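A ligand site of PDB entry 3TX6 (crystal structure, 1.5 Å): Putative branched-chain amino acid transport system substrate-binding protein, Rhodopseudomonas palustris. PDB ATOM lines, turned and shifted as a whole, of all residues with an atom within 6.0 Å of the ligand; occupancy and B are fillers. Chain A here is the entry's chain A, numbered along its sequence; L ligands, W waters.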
ATOM      1  N   LEU A  23      14.515  24.488 -34.222  1.00  0.00           N
ATOM      2  CA  LEU A  23      15.609  23.533 -34.102  1.00  0.00           C
ATOM      3  C   LEU A  23      16.018  23.005 -35.475  1.00  0.00           C
ATOM      4  O   LEU A  23      17.205  22.916 -35.790  1.00  0.00           O
ATOM      5  CB  LEU A  23      15.235  22.360 -33.182  1.00  0.00           C
ATOM      6  CG  LEU A  23      15.301  22.659 -31.685  1.00  0.00           C
ATOM      7  CD1 LEU A  23      14.273  23.731 -31.246  1.00  0.00           C
ATOM      8  CD2 LEU A  23      15.134  21.374 -30.871  1.00  0.00           C
ATOM      9  N   GLU A  27      19.484  23.371 -38.549  1.00  0.00           N
ATOM     10  CA  GLU A  27      20.050  22.091 -38.985  1.00  0.00           C
ATOM     11  C   GLU A  27      20.104  21.969 -40.489  1.00  0.00           C
ATOM     12  O   GLU A  27      21.126  21.517 -41.049  1.00  0.00           O
ATOM     13  CB  GLU A  27      19.277  20.944 -38.326  1.00  0.00           C
ATOM     14  CG  GLU A  27      19.594  20.888 -36.856  1.00  0.00           C
ATOM     15  CD  GLU A  27      18.734  20.031 -35.946  1.00  0.00           C
ATOM     16  OE1 GLU A  27      17.730  19.456 -36.366  1.00  0.00           O
ATOM     17  OE2 GLU A  27      19.115  19.986 -34.746  1.00  0.00           O
ATOM     18  N   SER A  77      14.964  16.328 -35.334  1.00  0.00           N
ATOM     19  CA  SER A  77      15.302  17.493 -34.521  1.00  0.00           C
ATOM     20  C   SER A  77      14.903  17.360 -33.035  1.00  0.00           C
ATOM     21  O   SER A  77      15.408  18.082 -32.172  1.00  0.00           O
ATOM     22  CB  SER A  77      14.618  18.744 -35.104  1.00  0.00           C
ATOM     23  OG  SER A  77      15.062  18.977 -36.447  1.00  0.00           O
ATOM     24  N   VAL A  78      13.918  16.526 -32.775  1.00  0.00           N
ATOM     25  CA  VAL A  78      13.363  16.325 -31.444  1.00  0.00           C
ATOM     26  C   VAL A  78      13.221  14.813 -31.234  1.00  0.00           C
ATOM     27  O   VAL A  78      13.309  14.038 -32.199  1.00  0.00           O
ATOM     28  CB  VAL A  78      12.061  17.126 -31.193  1.00  0.00           C
ATOM     29  CG1 VAL A  78      12.373  18.619 -31.068  1.00  0.00           C
ATOM     30  CG2 VAL A  78      11.024  16.832 -32.280  1.00  0.00           C
ATOM     31  N   THR A  79      13.066  14.419 -29.970  1.00  0.00           N
ATOM     32  CA  THR A  79      13.171  13.000 -29.625  1.00  0.00           C
ATOM     33  C   THR A  79      12.150  12.069 -30.277  1.00  0.00           C
ATOM     34  O   THR A  79      12.557  11.033 -30.808  1.00  0.00           O
ATOM     35  CB  THR A  79      13.261  12.788 -28.095  1.00  0.00           C
ATOM     36  OG1 THR A  79      14.420  13.488 -27.614  1.00  0.00           O
ATOM     37  CG2 THR A  79      13.337  11.311 -27.730  1.00  0.00           C
ATOM     38  N   PRO A  80      10.856  12.420 -30.278  1.00  0.00           N
ATOM     39  CA  PRO A  80       9.892  11.425 -30.804  1.00  0.00           C
ATOM     40  C   PRO A  80      10.149  11.008 -32.280  1.00  0.00           C
ATOM     41  O   PRO A  80      10.186   9.815 -32.569  1.00  0.00           O
ATOM     42  CB  PRO A  80       8.513  12.113 -30.583  1.00  0.00           C
ATOM     43  CG  PRO A  80       8.779  12.945 -29.348  1.00  0.00           C
ATOM     44  CD  PRO A  80      10.159  13.523 -29.622  1.00  0.00           C
ATOM     45  N   LEU A  99      20.090  13.522 -34.461  1.00  0.00           N
ATOM     46  CA  LEU A  99      20.284  14.956 -34.213  1.00  0.00           C
ATOM     47  C   LEU A  99      19.490  15.455 -32.980  1.00  0.00           C
ATOM     48  O   LEU A  99      19.480  16.656 -32.703  1.00  0.00           O
ATOM     49  CB  LEU A  99      19.985  15.756 -35.479  1.00  0.00           C
ATOM     50  CG  LEU A  99      20.784  15.405 -36.733  1.00  0.00           C
ATOM     51  CD1 LEU A  99      20.393  16.309 -37.930  1.00  0.00           C
ATOM     52  CD2 LEU A  99      22.312  15.410 -36.527  1.00  0.00           C
ATOM     53  N   ALA A 100      18.872  14.538 -32.230  1.00  0.00           N
ATOM     54  CA  ALA A 100      18.213  14.777 -30.955  1.00  0.00           C
ATOM     55  C   ALA A 100      18.593  13.653 -30.031  1.00  0.00           C
ATOM     56  O   ALA A 100      18.906  12.588 -30.496  1.00  0.00           O
ATOM     57  CB  ALA A 100      16.700  14.790 -31.104  1.00  0.00           C
ATOM     58  N   PRO A 101      18.719  13.962 -28.735  1.00  0.00           N
ATOM     59  CA  PRO A 101      19.014  12.881 -27.814  1.00  0.00           C
ATOM     60  C   PRO A 101      17.812  11.885 -27.890  1.00  0.00           C
ATOM     61  O   PRO A 101      16.679  12.239 -28.266  1.00  0.00           O
ATOM     62  CB  PRO A 101      19.271  13.574 -26.492  1.00  0.00           C
ATOM     63  CG  PRO A 101      18.685  14.901 -26.590  1.00  0.00           C
ATOM     64  CD  PRO A 101      18.452  15.229 -28.042  1.00  0.00           C
ATOM     65  N   PRO A 116      23.834  14.914 -30.241  1.00  0.00           N
ATOM     66  CA  PRO A 116      23.615  15.719 -29.017  1.00  0.00           C
ATOM     67  C   PRO A 116      24.233  15.087 -27.776  1.00  0.00           C
ATOM     68  O   PRO A 116      24.332  13.866 -27.673  1.00  0.00           O
ATOM     69  CB  PRO A 116      22.088  15.791 -28.895  1.00  0.00           C
ATOM     70  CG  PRO A 116      21.623  15.617 -30.305  1.00  0.00           C
ATOM     71  CD  PRO A 116      22.555  14.544 -30.845  1.00  0.00           C
ATOM     72  N   GLN A 117      24.650  15.944 -26.838  1.00  0.00           N
ATOM     73  CA  GLN A 117      25.141  15.478 -25.597  1.00  0.00           C
ATOM     74  C   GLN A 117      24.087  14.621 -24.867  1.00  0.00           C
ATOM     75  O   GLN A 117      22.917  14.973 -24.834  1.00  0.00           O
ATOM     76  CB  GLN A 117      25.532  16.652 -24.710  1.00  0.00           C
ATOM     77  CG  GLN A 117      26.698  17.482 -25.243  1.00  0.00           C
ATOM     78  CD  GLN A 117      26.332  18.470 -26.341  1.00  0.00           C
ATOM     79  OE1 GLN A 117      25.157  18.629 -26.674  1.00  0.00           O
ATOM     80  NE2 GLN A 117      27.348  19.194 -26.874  1.00  0.00           N
ATOM     81  N   TYR A 143       8.495  18.016 -20.346  1.00  0.00           N
ATOM     82  CA  TYR A 143       7.520  17.328 -21.202  1.00  0.00           C
ATOM     83  C   TYR A 143       7.046  16.029 -20.628  1.00  0.00           C
ATOM     84  O   TYR A 143       7.811  15.289 -19.982  1.00  0.00           O
ATOM     85  CB  TYR A 143       8.056  17.005 -22.600  1.00  0.00           C
ATOM     86  CG  TYR A 143       8.536  18.156 -23.442  1.00  0.00           C
ATOM     87  CD1 TYR A 143       7.808  19.336 -23.537  1.00  0.00           C
ATOM     88  CD2 TYR A 143       9.648  18.021 -24.244  1.00  0.00           C
ATOM     89  CE1 TYR A 143       8.248  20.371 -24.347  1.00  0.00           C
ATOM     90  CE2 TYR A 143      10.092  19.037 -25.043  1.00  0.00           C
ATOM     91  CZ  TYR A 143       9.371  20.209 -25.118  1.00  0.00           C
ATOM     92  OH  TYR A 143       9.811  21.235 -25.927  1.00  0.00           O
ATOM     93  N   ASP A 145       6.749  13.269 -22.138  1.00  0.00           N
ATOM     94  CA  ASP A 145       7.164  12.255 -23.156  1.00  0.00           C
ATOM     95  C   ASP A 145       8.610  11.809 -22.868  1.00  0.00           C
ATOM     96  O   ASP A 145       9.160  12.179 -21.847  1.00  0.00           O
ATOM     97  CB  ASP A 145       6.929  12.780 -24.578  1.00  0.00           C
ATOM     98  CG  ASP A 145       7.900  13.883 -25.009  1.00  0.00           C
ATOM     99  OD1 ASP A 145       8.894  14.150 -24.337  1.00  0.00           O
ATOM    100  OD2 ASP A 145       7.607  14.548 -26.020  1.00  0.00           O
ATOM    101  N   TYR A 147      11.613  12.563 -23.850  1.00  0.00           N
ATOM    102  CA  TYR A 147      12.617  13.596 -23.554  1.00  0.00           C
ATOM    103  C   TYR A 147      12.446  14.104 -22.126  1.00  0.00           C
ATOM    104  O   TYR A 147      13.426  14.212 -21.373  1.00  0.00           O
ATOM    105  CB  TYR A 147      12.526  14.762 -24.550  1.00  0.00           C
ATOM    106  CG  TYR A 147      13.584  15.854 -24.317  1.00  0.00           C
ATOM    107  CD1 TYR A 147      14.917  15.680 -24.705  1.00  0.00           C
ATOM    108  CD2 TYR A 147      13.248  17.056 -23.673  1.00  0.00           C
ATOM    109  CE1 TYR A 147      15.867  16.664 -24.478  1.00  0.00           C
ATOM    110  CE2 TYR A 147      14.194  18.049 -23.457  1.00  0.00           C
ATOM    111  CZ  TYR A 147      15.521  17.847 -23.827  1.00  0.00           C
ATOM    112  OH  TYR A 147      16.495  18.794 -23.638  1.00  0.00           O
ATOM    113  N   ARG A 174       4.053  19.161 -25.350  1.00  0.00           N
ATOM    114  CA  ARG A 174       4.729  20.058 -26.297  1.00  0.00           C
ATOM    115  C   ARG A 174       3.830  21.169 -26.847  1.00  0.00           C
ATOM    116  O   ARG A 174       4.262  22.326 -26.937  1.00  0.00           O
ATOM    117  CB  ARG A 174       5.335  19.269 -27.479  1.00  0.00           C
ATOM    118  CG  ARG A 174       6.527  18.423 -27.066  1.00  0.00           C
ATOM    119  CD  ARG A 174       7.028  17.523 -28.189  1.00  0.00           C
ATOM    120  NE  ARG A 174       8.047  16.645 -27.611  1.00  0.00           N
ATOM    121  CZ  ARG A 174       9.354  16.865 -27.644  1.00  0.00           C
ATOM    122  NH1 ARG A 174      10.136  16.031 -27.015  1.00  0.00           N
ATOM    123  NH2 ARG A 174       9.887  17.898 -28.308  1.00  0.00           N
ATOM    124  N   ALA A 198      12.600  20.851 -21.383  1.00  0.00           N
ATOM    125  CA  ALA A 198      11.847  21.162 -22.569  1.00  0.00           C
ATOM    126  C   ALA A 198      12.862  21.663 -23.609  1.00  0.00           C
ATOM    127  O   ALA A 198      14.072  21.530 -23.436  1.00  0.00           O
ATOM    128  CB  ALA A 198      10.771  22.180 -22.234  1.00  0.00           C
ATOM    129  N   SER A 199      12.368  22.219 -24.717  1.00  0.00           N
ATOM    130  CA  SER A 199      13.230  22.644 -25.824  1.00  0.00           C
ATOM    131  C   SER A 199      12.503  23.717 -26.606  1.00  0.00           C
ATOM    132  O   SER A 199      11.289  23.835 -26.523  1.00  0.00           O
ATOM    133  CB  SER A 199      13.545  21.466 -26.735  1.00  0.00           C
ATOM    134  OG  SER A 199      12.373  20.945 -27.311  1.00  0.00           O
ATOM    135  N   THR A 222      17.821  22.999 -20.037  1.00  0.00           N
ATOM    136  CA  THR A 222      18.554  22.003 -20.787  1.00  0.00           C
ATOM    137  C   THR A 222      19.123  22.530 -22.100  1.00  0.00           C
ATOM    138  O   THR A 222      18.846  23.652 -22.510  1.00  0.00           O
ATOM    139  CB  THR A 222      17.644  20.799 -21.134  1.00  0.00           C
ATOM    140  OG1 THR A 222      16.701  21.115 -22.176  1.00  0.00           O
ATOM    141  CG2 THR A 222      16.901  20.257 -19.899  1.00  0.00           C
ATOM    142  N   HIS A 223      19.909  21.678 -22.750  1.00  0.00           N
ATOM    143  CA  HIS A 223      20.552  22.028 -24.006  1.00  0.00           C
ATOM    144  C   HIS A 223      19.554  22.118 -25.159  1.00  0.00           C
ATOM    145  O   HIS A 223      19.888  22.649 -26.199  1.00  0.00           O
ATOM    146  CB  HIS A 223      21.760  21.148 -24.338  1.00  0.00           C
ATOM    147  CG  HIS A 223      21.517  19.646 -24.294  1.00  0.00           C
ATOM    148  ND1 HIS A 223      20.693  19.038 -23.399  1.00  0.00           N
ATOM    149  CD2 HIS A 223      22.164  18.621 -24.983  1.00  0.00           C
ATOM    150  CE1 HIS A 223      20.784  17.684 -23.602  1.00  0.00           C
ATOM    151  NE2 HIS A 223      21.672  17.452 -24.560  1.00  0.00           N
ATOM    152  N   GLY A 224      18.323  21.639 -24.939  1.00  0.00           N
ATOM    153  CA  GLY A 224      17.213  21.875 -25.867  1.00  0.00           C
ATOM    154  C   GLY A 224      16.805  23.326 -25.979  1.00  0.00           C
ATOM    155  O   GLY A 224      16.044  23.660 -26.924  1.00  0.00           O
ATOM    156  N   ALA A 225      17.348  24.180 -25.104  1.00  0.00           N
ATOM    157  CA  ALA A 225      17.054  25.621 -25.121  1.00  0.00           C
ATOM    158  C   ALA A 225      18.173  26.490 -25.748  1.00  0.00           C
ATOM    159  O   ALA A 225      18.000  27.688 -25.817  1.00  0.00           O
ATOM    160  CB  ALA A 225      16.751  26.137 -23.671  1.00  0.00           C
ATOM    161  N   GLN A 282      23.071  25.610 -30.852  1.00  0.00           N
ATOM    162  CA  GLN A 282      23.211  24.181 -30.498  1.00  0.00           C
ATOM    163  C   GLN A 282      22.887  23.287 -31.679  1.00  0.00           C
ATOM    164  O   GLN A 282      23.576  22.302 -31.931  1.00  0.00           O
ATOM    165  CB  GLN A 282      22.250  23.886 -29.344  1.00  0.00           C
ATOM    166  CG  GLN A 282      22.203  22.457 -28.813  1.00  0.00           C
ATOM    167  CD  GLN A 282      23.400  22.034 -27.975  1.00  0.00           C
ATOM    168  OE1 GLN A 282      24.271  22.854 -27.639  1.00  0.00           O
ATOM    169  NE2 GLN A 282      23.428  20.757 -27.637  1.00  0.00           N
ATOM    170  N   PHE A 283      21.832  23.642 -32.394  1.00  0.00           N
ATOM    171  CA  PHE A 283      21.192  22.736 -33.363  1.00  0.00           C
ATOM    172  C   PHE A 283      21.910  22.696 -34.721  1.00  0.00           C
ATOM    173  O   PHE A 283      22.200  21.612 -35.262  1.00  0.00           O
ATOM    174  CB  PHE A 283      19.698  23.135 -33.493  1.00  0.00           C
ATOM    175  CG  PHE A 283      19.090  23.314 -32.134  1.00  0.00           C
ATOM    176  CD1 PHE A 283      18.983  22.253 -31.297  1.00  0.00           C
ATOM    177  CD2 PHE A 283      18.705  24.582 -31.675  1.00  0.00           C
ATOM    178  CE1 PHE A 283      18.554  22.407 -29.999  1.00  0.00           C
ATOM    179  CE2 PHE A 283      18.236  24.748 -30.372  1.00  0.00           C
ATOM    180  CZ  PHE A 283      18.151  23.647 -29.528  1.00  0.00           C
ATOM    181  N   HIS A 286      24.770  20.316 -34.673  1.00  0.00           N
ATOM    182  CA  HIS A 286      24.605  18.863 -34.767  1.00  0.00           C
ATOM    183  C   HIS A 286      24.660  18.358 -36.190  1.00  0.00           C
ATOM    184  O   HIS A 286      25.298  17.337 -36.427  1.00  0.00           O
ATOM    185  CB  HIS A 286      23.353  18.362 -34.065  1.00  0.00           C
ATOM    186  CG  HIS A 286      23.297  18.669 -32.605  1.00  0.00           C
ATOM    187  ND1 HIS A 286      24.375  18.575 -31.758  1.00  0.00           N
ATOM    188  CD2 HIS A 286      22.224  19.093 -31.824  1.00  0.00           C
ATOM    189  CE1 HIS A 286      23.965  18.905 -30.502  1.00  0.00           C
ATOM    190  NE2 HIS A 286      22.674  19.220 -30.543  1.00  0.00           N
ATOM    191  N   GLN A 330      30.817  20.421 -31.228  1.00  0.00           N
ATOM    192  CA  GLN A 330      30.122  20.164 -29.962  1.00  0.00           C
ATOM    193  C   GLN A 330      30.829  19.219 -28.992  1.00  0.00           C
ATOM    194  O   GLN A 330      30.343  18.995 -27.884  1.00  0.00           O
ATOM    195  CB  GLN A 330      28.707  19.648 -30.260  1.00  0.00           C
ATOM    196  CG  GLN A 330      27.833  20.689 -30.943  1.00  0.00           C
ATOM    197  CD  GLN A 330      27.309  21.722 -29.957  1.00  0.00           C
ATOM    198  OE1 GLN A 330      28.117  22.326 -29.228  1.00  0.00           O
ATOM    199  NE2 GLN A 330      25.975  21.925 -29.868  1.00  0.00           N
HETATM  200  O1  LIG L   1      15.406  16.197 -28.191  1.00  0.00           O
HETATM  201  C1  LIG L   1      17.572  18.569 -29.333  1.00  0.00           C
HETATM  202  C2  LIG L   1      18.937  18.695 -29.444  1.00  0.00           C
HETATM  203  C3  LIG L   1      19.735  18.892 -28.309  1.00  0.00           C
HETATM  204  C4  LIG L   1      19.136  18.861 -27.069  1.00  0.00           C
HETATM  205  C5  LIG L   1      17.748  18.759 -26.940  1.00  0.00           C
HETATM  206  C6  LIG L   1      16.947  18.600 -28.089  1.00  0.00           C
HETATM  207  O2  LIG L   1      21.120  18.981 -28.468  1.00  0.00           O
HETATM  208  C7  LIG L   1      15.450  18.549 -27.975  1.00  0.00           C
HETATM  209  C8  LIG L   1      14.768  17.238 -27.957  1.00  0.00           C
HETATM  210  C9  LIG L   1      13.330  17.234 -27.786  1.00  0.00           C
HETATM  211  O3  LIG L   1      12.742  16.124 -27.822  1.00  0.00           O
HETATM  212  O4  LIG L   1      12.688  18.309 -27.598  1.00  0.00           O
HETATM  213  O   HOH W   1      17.973  18.829 -32.793  1.00  0.00           O
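NH1 of Arg 174 is in salt-bridge range of O3 of the ligand (2.7 Å).
OG1 of Thr 79 sits at hydrogen-bond distance from O1 of the ligand, 2.9 Å away.
OG of Ser 199 sits at hydrogen-bond distance from O4 of the ligand, at 2.7 Å.
An oxygen (O3) of the ligand is in hydrogen-bond range of the backbone NH of Thr 79 (2.8 Å).
An oxygen (O2) of the ligand is in hydrogen-bond range of a ring nitrogen (NE2) of His 286 (2.6 Å).
An oxygen (O2) of the ligand lies within hydrogen-bond range of the side-chain amide nitrogen (NE2) of Gln 282 (3.0 Å).
O of Ser 77 touches C1 of the ligand, 3.6 Å away.
Val 78 touches the ligand (CG1 to O4, 3.5 Å).
O of Leu 99 touches C2 of the ligand, at 3.9 Å.
Ala 100 touches the ligand.
Pro 101 touches the ligand.
Pro 116 touches the ligand.
CE2 of Tyr 143 touches O4 of the ligand, at 3.7 Å.
OH of Tyr 147 touches C5 of the ligand (3.5 Å).
His 223 touches the ligand.
CA of Gly 224 touches C5 of the ligand (3.3 Å).
Phe 283 touches the ligand.
Hydrophobic or aromatic side chains that line the ligand: Val 78, Ala 100, Pro 101, Pro 116, Tyr 143, Tyr 147, His 223, Phe 283 and His 286.
16 residues have an atom within 4 Å of the ligand: Ser 77, Val 78, Thr 79, Leu 99, Ala 100, Pro 101, Pro 116, Tyr 143, Tyr 147, Arg 174, Ser 199, His 223, Gly 224, Gln 282, Phe 283 and His 286.
The nearest printed residue that does not touch the ligand is Leu 23 (4.02 Å).
NE2 of Gln 282 sits at hydrogen-bond distance from OE1 of Gln 117 (2.9 Å).
A ring nitrogen (NE2) of His 223 is in hydrogen-bond range of the backbone carbonyl oxygen of Gln 117 (2.8 Å).
OG of Ser 199 sits at hydrogen-bond distance from OH of Tyr 143.
The side-chain amide oxygen of Gln 282 lies within hydrogen-bond range of the side-chain amide nitrogen of Gln 330 (3.0 Å).
N of Gly 224 lies close to OG1 of Thr 222.
The side-chain hydroxyl (OG1) of Thr 79 sits at hydrogen-bond distance from the backbone carbonyl oxygen (O) of Pro 101 (2.7 Å).
The guanidinium group (NE) of Arg 174 lies within salt-bridge range of the side-chain carboxylate (OD2) of Asp 145 (2.7 Å).
The backbone NH (N) of Tyr 147 lies within hydrogen-bond range of the side-chain carboxylate (OD1) of Asp 145 (3.2 Å).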
